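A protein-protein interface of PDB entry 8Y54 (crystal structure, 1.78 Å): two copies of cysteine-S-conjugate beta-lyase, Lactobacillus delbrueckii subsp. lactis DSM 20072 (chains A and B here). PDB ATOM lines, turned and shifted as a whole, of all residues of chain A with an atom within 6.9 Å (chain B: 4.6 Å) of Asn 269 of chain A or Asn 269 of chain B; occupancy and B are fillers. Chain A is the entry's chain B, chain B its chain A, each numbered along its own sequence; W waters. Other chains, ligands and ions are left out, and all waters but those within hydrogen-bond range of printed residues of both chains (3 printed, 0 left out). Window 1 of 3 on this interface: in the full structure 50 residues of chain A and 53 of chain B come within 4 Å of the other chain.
N of Leu 270 of chain B is in hydrogen-bond range of O of Ala 239 of chain A (2.8 Å). The backbone carbonyl oxygen of Ala 239 of chain B lies within hydrogen-bond range of the backbone NH of Leu 270 of chain A, at 2.8 Å. ND2 of Asn 17 of chain A sits at hydrogen-bond distance from OE2 of Glu 60 of chain B (2.7 Å). A ring nitrogen (NE2) of His 241 of chain A lies within hydrogen-bond range of the side-chain carboxylate (OE1) of Glu 267 of chain B (3.0 Å).
The backbone carbonyl oxygen (O) of Leu 240 of chain B sits at hydrogen-bond distance from the side-chain amide nitrogen (ND2) of Asn 269 of chain B (2.9 Å). N of Leu 271 of chain B sits at hydrogen-bond distance from OD1 of Asn 269 of chain B. ND2 of Asn 269 of chain A sits at hydrogen-bond distance from O of Leu 240 of chain A (2.8 Å). The backbone carbonyl oxygen (O) of Glu 267 of chain A lies within hydrogen-bond range of the side-chain hydroxyl (OG) of Ser 91 of chain A (3.4 Å). The side-chain amide oxygen (OD1) of Asn 269 of chain B sits at hydrogen-bond distance from the backbone NH (N) of Ala 272 of chain B, 3.0 Å away. The backbone carbonyl oxygen (O) of Leu 270 of chain A is in hydrogen-bond range of the side-chain amino group (NZ) of Lys 51 of chain A (2.8 Å).
Among the printed residues, pairs that only touch across the chains: Gly 58 of chain A with Ala 239 of chain B (3.2 Å), Ala 239 of chain A with Asn 269 of chain B (3.2 Å), His 241 of chain A with Pro 268 of chain B (3.6 Å), His 241 of chain A with Asn 269 of chain B (3.5 Å), Glu 267 of chain A with His 241 of chain B (3.2 Å), Pro 268 of chain A with His 241 of chain B (3.6 Å), Asn 269 of chain A with Ala 239 of chain B (3.2 Å), Asn 269 of chain A with His 241 of chain B (3.5 Å), Asn 269 of chain A with Asn 269 of chain B (3.5 Å), Leu 270 of chain A with Leu 271 of chain B (3.9 Å), Leu 271 of chain A with Leu 270 of chain B (3.8 Å) and Leu 271 of chain A with Leu 271 of chain B (3.6 Å).
Asn 269 of chain B touches just these residues of chain A: Ala 239 (3.2 Å), His 241 (3.5 Å) and Asn 269 (3.5 Å). Of the printed residues of chain B, Ala 239 of chain A touches Asn 269 and Leu 270. Printed residues of chain B within 4 Å of Asn 17 of chain A: Glu 60 (2.7 Å). Ala 272 of chain A touches none of the printed residues of chain B. The nearest printed residue of chain B that does not touch Asn 269 of chain A is Leu 240 of chain B (4.6 Å). The nearest residue of chain A that does not touch Asn 269 of chain B is Leu 240 of chain A (4.7 Å). The nearest printed residue of chain A that does not touch Glu 267 of chain B is Ala 238 of chain A (4.4 Å).
Of the 19 printed residues of chain A, 9 touch a printed residue of chain B. Among the printed residues, 16 pairs touch across the chains. Among the printed residues, no Asp or Glu carboxylate lies within 4 Å of a Lys or Arg side-chain nitrogen of the other chain.
Ala 239 of chain A touches Asn 269 of chain B, and with the chains exchanged Asn 269 of chain A touches Ala 239 of chain B. His 241 of chain A touches Pro 268 of chain B, and with the chains exchanged Pro 268 of chain A touches His 241 of chain B. His 241 of chain A touches Asn 269 of chain B, and with the chains exchanged Asn 269 of chain A touches His 241 of chain B. Leu 270 of chain A touches Leu 271 of chain B, and with the chains exchanged Leu 271 of chain A touches Leu 270 of chain B. Of the 16 pairs that touch across the chains among the printed residues, 14 have their exchanged pair printed and touching as well.
Water W2 bridges the side-chain carboxylate of Glu 267 of chain A (2.6 Å) and a ring nitrogen (NE2) of His 241 of chain B (2.9 Å). Water W3 lies within hydrogen-bond range of a ring nitrogen (ND1) of His 241 of chain B, the side-chain amide nitrogen of Asn 269 of chain A and the side-chain amide nitrogen of Asn 269 of chain B. Water W1 bridges O of Ala 238 of chain A (2.9 Å) and OE1 of Glu 267 of chain B (3.1 Å).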
ATOM      1  N   ASN A  17      38.236 -12.625 -27.332  1.00  0.00           N
ATOM      2  CA  ASN A  17      38.301 -13.327 -26.053  1.00  0.00           C
ATOM      3  C   ASN A  17      37.881 -14.794 -26.154  1.00  0.00           C
ATOM      4  O   ASN A  17      37.498 -15.395 -25.145  1.00  0.00           O
ATOM      5  CB  ASN A  17      37.453 -12.607 -24.999  1.00  0.00           C
ATOM      6  CG  ASN A  17      35.964 -12.725 -25.263  1.00  0.00           C
ATOM      7  OD1 ASN A  17      35.526 -12.604 -26.401  1.00  0.00           O
ATOM      8  ND2 ASN A  17      35.175 -12.958 -24.200  1.00  0.00           N
ATOM      9  N   LYS A  51      14.621 -12.831 -29.420  1.00  0.00           N
ATOM     10  CA  LYS A  51      14.651 -12.476 -28.012  1.00  0.00           C
ATOM     11  C   LYS A  51      15.316 -11.121 -27.808  1.00  0.00           C
ATOM     12  O   LYS A  51      14.929 -10.355 -26.915  1.00  0.00           O
ATOM     13  CB  LYS A  51      15.377 -13.578 -27.224  1.00  0.00           C
ATOM     14  CG  LYS A  51      15.567 -13.288 -25.731  1.00  0.00           C
ATOM     15  CD  LYS A  51      14.245 -12.995 -25.030  1.00  0.00           C
ATOM     16  CE  LYS A  51      14.410 -12.764 -23.525  1.00  0.00           C
ATOM     17  NZ  LYS A  51      14.820 -14.013 -22.784  1.00  0.00           N
ATOM     18  N   GLY A  58      15.397  -8.107 -17.927  1.00  0.00           N
ATOM     19  CA  GLY A  58      15.146  -8.312 -16.520  1.00  0.00           C
ATOM     20  C   GLY A  58      15.107  -9.787 -16.187  1.00  0.00           C
ATOM     21  O   GLY A  58      15.553 -10.642 -16.954  1.00  0.00           O
ATOM     22  N   GLU A  60      14.258 -13.626 -15.428  1.00  0.00           N
ATOM     23  CA  GLU A  60      13.554 -14.653 -16.187  1.00  0.00           C
ATOM     24  C   GLU A  60      13.100 -15.812 -15.310  1.00  0.00           C
ATOM     25  O   GLU A  60      13.848 -16.268 -14.443  1.00  0.00           O
ATOM     26  CB  GLU A  60      14.459 -15.226 -17.265  1.00  0.00           C
ATOM     27  CG  GLU A  60      15.155 -14.205 -18.097  1.00  0.00           C
ATOM     28  CD  GLU A  60      14.913 -14.455 -19.564  1.00  0.00           C
ATOM     29  OE1 GLU A  60      15.184 -13.526 -20.346  1.00  0.00           O
ATOM     30  OE2 GLU A  60      14.455 -15.582 -19.920  1.00  0.00           O
ATOM     31  N   PHE A  89      16.157 -26.603 -14.633  1.00  0.00           N
ATOM     32  CA  PHE A  89      17.156 -25.780 -15.316  1.00  0.00           C
ATOM     33  C   PHE A  89      18.405 -25.567 -14.462  1.00  0.00           C
ATOM     34  O   PHE A  89      18.327 -25.323 -13.254  1.00  0.00           O
ATOM     35  CB  PHE A  89      16.568 -24.413 -15.691  1.00  0.00           C
ATOM     36  CG  PHE A  89      17.554 -23.508 -16.391  1.00  0.00           C
ATOM     37  CD1 PHE A  89      18.384 -22.660 -15.665  1.00  0.00           C
ATOM     38  CD2 PHE A  89      17.678 -23.538 -17.766  1.00  0.00           C
ATOM     39  CE1 PHE A  89      19.311 -21.837 -16.304  1.00  0.00           C
ATOM     40  CE2 PHE A  89      18.600 -22.722 -18.413  1.00  0.00           C
ATOM     41  CZ  PHE A  89      19.419 -21.873 -17.678  1.00  0.00           C
ATOM     42  N   SER A  91      22.483 -23.526 -15.123  1.00  0.00           N
ATOM     43  CA  SER A  91      23.227 -22.732 -16.099  1.00  0.00           C
ATOM     44  C   SER A  91      24.396 -23.479 -16.732  1.00  0.00           C
ATOM     45  O   SER A  91      25.037 -22.949 -17.647  1.00  0.00           O
ATOM     46  CB  SER A  91      23.719 -21.431 -15.460  1.00  0.00           C
ATOM     47  OG  SER A  91      22.627 -20.542 -15.308  1.00  0.00           O
ATOM     48  N   ALA A 238      28.534 -23.575 -25.964  1.00  0.00           N
ATOM     49  CA  ALA A 238      29.154 -23.658 -24.629  1.00  0.00           C
ATOM     50  C   ALA A 238      28.819 -22.420 -23.802  1.00  0.00           C
ATOM     51  O   ALA A 238      28.458 -22.558 -22.646  1.00  0.00           O
ATOM     52  CB  ALA A 238      30.636 -23.780 -24.744  1.00  0.00           C
ATOM     53  N   ALA A 239      28.965 -21.257 -24.410  1.00  0.00           N
ATOM     54  CA  ALA A 239      28.760 -20.030 -23.656  1.00  0.00           C
ATOM     55  C   ALA A 239      27.291 -19.669 -23.516  1.00  0.00           C
ATOM     56  O   ALA A 239      26.983 -18.650 -22.898  1.00  0.00           O
ATOM     57  CB  ALA A 239      29.531 -18.877 -24.297  1.00  0.00           C
ATOM     58  N   LEU A 240      26.369 -20.466 -24.059  1.00  0.00           N
ATOM     59  CA  LEU A 240      24.964 -20.159 -23.822  1.00  0.00           C
ATOM     60  C   LEU A 240      24.603 -20.332 -22.354  1.00  0.00           C
ATOM     61  O   LEU A 240      23.690 -19.661 -21.860  1.00  0.00           O
ATOM     62  CB  LEU A 240      24.063 -21.041 -24.672  1.00  0.00           C
ATOM     63  CG  LEU A 240      22.577 -20.781 -24.472  1.00  0.00           C
ATOM     64  CD1 LEU A 240      22.226 -19.361 -24.926  1.00  0.00           C
ATOM     65  CD2 LEU A 240      21.785 -21.838 -25.236  1.00  0.00           C
ATOM     66  N   HIS A 241      25.304 -21.218 -21.653  1.00  0.00           N
ATOM     67  CA  HIS A 241      25.036 -21.507 -20.245  1.00  0.00           C
ATOM     68  C   HIS A 241      23.579 -21.912 -20.034  1.00  0.00           C
ATOM     69  O   HIS A 241      22.853 -21.350 -19.207  1.00  0.00           O
ATOM     70  CB  HIS A 241      25.422 -20.330 -19.349  1.00  0.00           C
ATOM     71  CG  HIS A 241      26.902 -20.102 -19.271  1.00  0.00           C
ATOM     72  ND1 HIS A 241      27.466 -19.131 -18.473  1.00  0.00           N
ATOM     73  CD2 HIS A 241      27.933 -20.722 -19.896  1.00  0.00           C
ATOM     74  CE1 HIS A 241      28.780 -19.154 -18.614  1.00  0.00           C
ATOM     75  NE2 HIS A 241      29.091 -20.110 -19.474  1.00  0.00           N
ATOM     76  N   ALA A 242      23.167 -22.926 -20.783  1.00  0.00           N
ATOM     77  CA  ALA A 242      21.869 -23.559 -20.629  1.00  0.00           C
ATOM     78  C   ALA A 242      22.088 -25.050 -20.439  1.00  0.00           C
ATOM     79  O   ALA A 242      22.830 -25.672 -21.211  1.00  0.00           O
ATOM     80  CB  ALA A 242      20.983 -23.313 -21.853  1.00  0.00           C
ATOM     81  N   GLU A 267      19.150 -19.520 -12.408  1.00  0.00           N
ATOM     82  CA  GLU A 267      18.375 -18.534 -13.177  1.00  0.00           C
ATOM     83  C   GLU A 267      18.900 -18.444 -14.603  1.00  0.00           C
ATOM     84  O   GLU A 267      20.118 -18.300 -14.797  1.00  0.00           O
ATOM     85  CB  GLU A 267      18.448 -17.149 -12.531  1.00  0.00           C
ATOM     86  CG  GLU A 267      17.886 -17.081 -11.106  1.00  0.00           C
ATOM     87  CD  GLU A 267      17.625 -15.646 -10.655  1.00  0.00           C
ATOM     88  OE1 GLU A 267      16.828 -15.458  -9.708  1.00  0.00           O
ATOM     89  OE2 GLU A 267      18.205 -14.710 -11.255  1.00  0.00           O
ATOM     90  N   PRO A 268      18.042 -18.495 -15.618  1.00  0.00           N
ATOM     91  CA  PRO A 268      18.546 -18.404 -16.991  1.00  0.00           C
ATOM     92  C   PRO A 268      18.981 -16.990 -17.313  1.00  0.00           C
ATOM     93  O   PRO A 268      18.370 -16.010 -16.868  1.00  0.00           O
ATOM     94  CB  PRO A 268      17.349 -18.830 -17.850  1.00  0.00           C
ATOM     95  CG  PRO A 268      16.151 -18.686 -16.979  1.00  0.00           C
ATOM     96  CD  PRO A 268      16.603 -18.799 -15.556  1.00  0.00           C
ATOM     97  N   ASN A 269      20.039 -16.894 -18.114  1.00  0.00           N
ATOM     98  CA  ASN A 269      20.398 -15.612 -18.694  1.00  0.00           C
ATOM     99  C   ASN A 269      19.417 -15.269 -19.817  1.00  0.00           C
ATOM    100  O   ASN A 269      18.468 -16.006 -20.106  1.00  0.00           O
ATOM    101  CB  ASN A 269      21.850 -15.612 -19.188  1.00  0.00           C
ATOM    102  CG  ASN A 269      22.099 -16.579 -20.345  1.00  0.00           C
ATOM    103  OD1 ASN A 269      21.401 -16.557 -21.363  1.00  0.00           O
ATOM    104  ND2 ASN A 269      23.129 -17.415 -20.199  1.00  0.00           N
ATOM    105  N   LEU A 270      19.626 -14.103 -20.414  1.00  0.00           N
ATOM    106  CA  LEU A 270      18.706 -13.502 -21.415  1.00  0.00           C
ATOM    107  C   LEU A 270      18.493 -14.300 -22.709  1.00  0.00           C
ATOM    108  O   LEU A 270      17.561 -13.974 -23.423  1.00  0.00           O
ATOM    109  CB  LEU A 270      19.223 -12.086 -21.706  1.00  0.00           C
ATOM    110  CG  LEU A 270      20.446 -11.901 -22.617  1.00  0.00           C
ATOM    111  CD1 LEU A 270      20.760 -10.428 -22.768  1.00  0.00           C
ATOM    112  CD2 LEU A 270      21.700 -12.607 -22.120  1.00  0.00           C
ATOM    113  N   LEU A 271      19.359 -15.252 -23.005  1.00  0.00           N
ATOM    114  CA  LEU A 271      19.164 -16.053 -24.208  1.00  0.00           C
ATOM    115  C   LEU A 271      18.960 -17.539 -23.931  1.00  0.00           C
ATOM    116  O   LEU A 271      18.568 -18.269 -24.847  1.00  0.00           O
ATOM    117  CB  LEU A 271      20.355 -15.883 -25.169  1.00  0.00           C
ATOM    118  CG  LEU A 271      20.554 -14.508 -25.808  1.00  0.00           C
ATOM    119  CD1 LEU A 271      21.805 -14.504 -26.698  1.00  0.00           C
ATOM    120  CD2 LEU A 271      19.308 -14.096 -26.600  1.00  0.00           C
ATOM    121  N   ALA A 272      19.188 -18.001 -22.697  1.00  0.00           N
ATOM    122  CA  ALA A 272      19.245 -19.435 -22.424  1.00  0.00           C
ATOM    123  C   ALA A 272      17.950 -20.149 -22.802  1.00  0.00           C
ATOM    124  O   ALA A 272      17.979 -21.215 -23.424  1.00  0.00           O
ATOM    125  CB  ALA A 272      19.565 -19.665 -20.937  1.00  0.00           C
ATOM    126  N   ILE A 273      16.804 -19.604 -22.398  1.00  0.00           N
ATOM    127  CA  ILE A 273      15.512 -20.272 -22.609  1.00  0.00           C
ATOM    128  C   ILE A 273      15.137 -20.319 -24.095  1.00  0.00           C
ATOM    129  O   ILE A 273      14.991 -21.424 -24.650  1.00  0.00           O
ATOM    130  CB  ILE A 273      14.408 -19.599 -21.771  1.00  0.00           C
ATOM    131  CG1 ILE A 273      14.698 -19.739 -20.270  1.00  0.00           C
ATOM    132  CG2 ILE A 273      13.026 -20.153 -22.142  1.00  0.00           C
ATOM    133  CD1 ILE A 273      14.958 -21.191 -19.803  1.00  0.00           C
ATOM    134  N   PRO A 274      14.961 -19.190 -24.798  1.00  0.00           N
ATOM    135  CA  PRO A 274      14.545 -19.315 -26.209  1.00  0.00           C
ATOM    136  C   PRO A 274      15.541 -20.085 -27.065  1.00  0.00           C
ATOM    137  O   PRO A 274      15.132 -20.837 -27.957  1.00  0.00           O
ATOM    138  CB  PRO A 274      14.389 -17.851 -26.667  1.00  0.00           C
ATOM    139  CG  PRO A 274      15.174 -17.042 -25.714  1.00  0.00           C
ATOM    140  CD  PRO A 274      15.080 -17.774 -24.392  1.00  0.00           C
ATOM    141  N   GLU B  60      34.552 -18.701 -23.456  1.00  0.00           N
ATOM    142  CA  GLU B  60      35.025 -17.328 -23.426  1.00  0.00           C
ATOM    143  C   GLU B  60      35.964 -17.110 -22.262  1.00  0.00           C
ATOM    144  O   GLU B  60      35.754 -17.653 -21.175  1.00  0.00           O
ATOM    145  CB  GLU B  60      33.853 -16.375 -23.337  1.00  0.00           C
ATOM    146  CG  GLU B  60      33.082 -16.485 -24.600  1.00  0.00           C
ATOM    147  CD  GLU B  60      32.365 -15.234 -24.972  1.00  0.00           C
ATOM    148  OE1 GLU B  60      31.446 -15.360 -25.795  1.00  0.00           O
ATOM    149  OE2 GLU B  60      32.718 -14.155 -24.445  1.00  0.00           O
ATOM    150  N   ALA B 239      19.421 -10.123 -16.483  1.00  0.00           N
ATOM    151  CA  ALA B 239      19.624 -11.438 -17.076  1.00  0.00           C
ATOM    152  C   ALA B 239      20.881 -11.508 -17.925  1.00  0.00           C
ATOM    153  O   ALA B 239      21.116 -12.537 -18.569  1.00  0.00           O
ATOM    154  CB  ALA B 239      18.402 -11.861 -17.899  1.00  0.00           C
ATOM    155  N   LEU B 240      21.709 -10.457 -17.915  1.00  0.00           N
ATOM    156  CA  LEU B 240      22.983 -10.515 -18.625  1.00  0.00           C
ATOM    157  C   LEU B 240      23.975 -11.413 -17.903  1.00  0.00           C
ATOM    158  O   LEU B 240      24.765 -12.121 -18.543  1.00  0.00           O
ATOM    159  CB  LEU B 240      23.583  -9.117 -18.773  1.00  0.00           C
ATOM    160  CG  LEU B 240      24.953  -9.099 -19.464  1.00  0.00           C
ATOM    161  CD1 LEU B 240      24.849  -9.785 -20.828  1.00  0.00           C
ATOM    162  CD2 LEU B 240      25.514  -7.676 -19.622  1.00  0.00           C
ATOM    163  N   HIS B 241      23.980 -11.353 -16.572  1.00  0.00           N
ATOM    164  CA  HIS B 241      24.871 -12.165 -15.738  1.00  0.00           C
ATOM    165  C   HIS B 241      26.329 -11.749 -15.941  1.00  0.00           C
ATOM    166  O   HIS B 241      27.213 -12.575 -16.175  1.00  0.00           O
ATOM    167  CB  HIS B 241      24.670 -13.662 -15.988  1.00  0.00           C
ATOM    168  CG  HIS B 241      23.317 -14.155 -15.577  1.00  0.00           C
ATOM    169  ND1 HIS B 241      22.891 -15.445 -15.804  1.00  0.00           N
ATOM    170  CD2 HIS B 241      22.285 -13.519 -14.973  1.00  0.00           C
ATOM    171  CE1 HIS B 241      21.656 -15.584 -15.353  1.00  0.00           C
ATOM    172  NE2 HIS B 241      21.262 -14.429 -14.849  1.00  0.00           N
ATOM    173  N   GLU B 267      32.876 -17.929 -15.318  1.00  0.00           N
ATOM    174  CA  GLU B 267      33.038 -17.969 -16.767  1.00  0.00           C
ATOM    175  C   GLU B 267      31.950 -17.146 -17.422  1.00  0.00           C
ATOM    176  O   GLU B 267      30.766 -17.374 -17.135  1.00  0.00           O
ATOM    177  CB  GLU B 267      32.965 -19.415 -17.282  1.00  0.00           C
ATOM    178  CG  GLU B 267      32.908 -19.537 -18.827  1.00  0.00           C
ATOM    179  CD  GLU B 267      32.730 -20.968 -19.283  1.00  0.00           C
ATOM    180  OE1 GLU B 267      31.779 -21.259 -20.060  1.00  0.00           O
ATOM    181  OE2 GLU B 267      33.544 -21.807 -18.836  1.00  0.00           O
ATOM    182  N   PRO B 268      32.281 -16.194 -18.293  1.00  0.00           N
ATOM    183  CA  PRO B 268      31.221 -15.369 -18.886  1.00  0.00           C
ATOM    184  C   PRO B 268      30.403 -16.155 -19.892  1.00  0.00           C
ATOM    185  O   PRO B 268      30.917 -17.038 -20.585  1.00  0.00           O
ATOM    186  CB  PRO B 268      31.982 -14.213 -19.546  1.00  0.00           C
ATOM    187  CG  PRO B 268      33.391 -14.694 -19.703  1.00  0.00           C
ATOM    188  CD  PRO B 268      33.632 -15.707 -18.610  1.00  0.00           C
ATOM    189  N   ASN B 269      29.104 -15.851 -19.938  1.00  0.00           N
ATOM    190  CA  ASN B 269      28.237 -16.408 -20.965  1.00  0.00           C
ATOM    191  C   ASN B 269      28.494 -15.657 -22.274  1.00  0.00           C
ATOM    192  O   ASN B 269      29.400 -14.826 -22.378  1.00  0.00           O
ATOM    193  CB  ASN B 269      26.767 -16.390 -20.511  1.00  0.00           C
ATOM    194  CG  ASN B 269      26.191 -14.984 -20.367  1.00  0.00           C
ATOM    195  OD1 ASN B 269      26.500 -14.086 -21.147  1.00  0.00           O
ATOM    196  ND2 ASN B 269      25.325 -14.797 -19.367  1.00  0.00           N
ATOM    197  N   LEU B 270      27.681 -15.945 -23.285  1.00  0.00           N
ATOM    198  CA  LEU B 270      27.909 -15.425 -24.662  1.00  0.00           C
ATOM    199  C   LEU B 270      27.789 -13.906 -24.844  1.00  0.00           C
ATOM    200  O   LEU B 270      28.254 -13.438 -25.859  1.00  0.00           O
ATOM    201  CB  LEU B 270      27.033 -16.200 -25.657  1.00  0.00           C
ATOM    202  CG  LEU B 270      25.538 -15.883 -25.734  1.00  0.00           C
ATOM    203  CD1 LEU B 270      24.888 -16.747 -26.796  1.00  0.00           C
ATOM    204  CD2 LEU B 270      24.813 -16.085 -24.411  1.00  0.00           C
ATOM    205  N   LEU B 271      27.157 -13.195 -23.926  1.00  0.00           N
ATOM    206  CA  LEU B 271      26.955 -11.737 -24.149  1.00  0.00           C
ATOM    207  C   LEU B 271      27.599 -10.920 -23.032  1.00  0.00           C
ATOM    208  O   LEU B 271      27.830  -9.758 -23.233  1.00  0.00           O
ATOM    209  CB  LEU B 271      25.456 -11.452 -24.220  1.00  0.00           C
ATOM    210  CG  LEU B 271      24.746 -11.908 -25.489  1.00  0.00           C
ATOM    211  CD1 LEU B 271      23.295 -11.469 -25.475  1.00  0.00           C
ATOM    212  CD2 LEU B 271      25.445 -11.369 -26.718  1.00  0.00           C
ATOM    213  N   ALA B 272      27.919 -11.564 -21.911  1.00  0.00           N
ATOM    214  CA  ALA B 272      28.419 -10.833 -20.731  1.00  0.00           C
ATOM    215  C   ALA B 272      29.581  -9.893 -21.056  1.00  0.00           C
ATOM    216  O   ALA B 272      29.529  -8.749 -20.645  1.00  0.00           O
ATOM    217  CB  ALA B 272      28.793 -11.787 -19.638  1.00  0.00           C
HETATM  218  O   HOH W   1      30.163 -23.791 -20.721  1.00  0.00           O
HETATM  219  O   HOH W   2      18.956 -13.504 -13.429  1.00  0.00           O
HETATM  220  O   HOH W   3      24.382 -17.006 -17.385  1.00  0.00           O
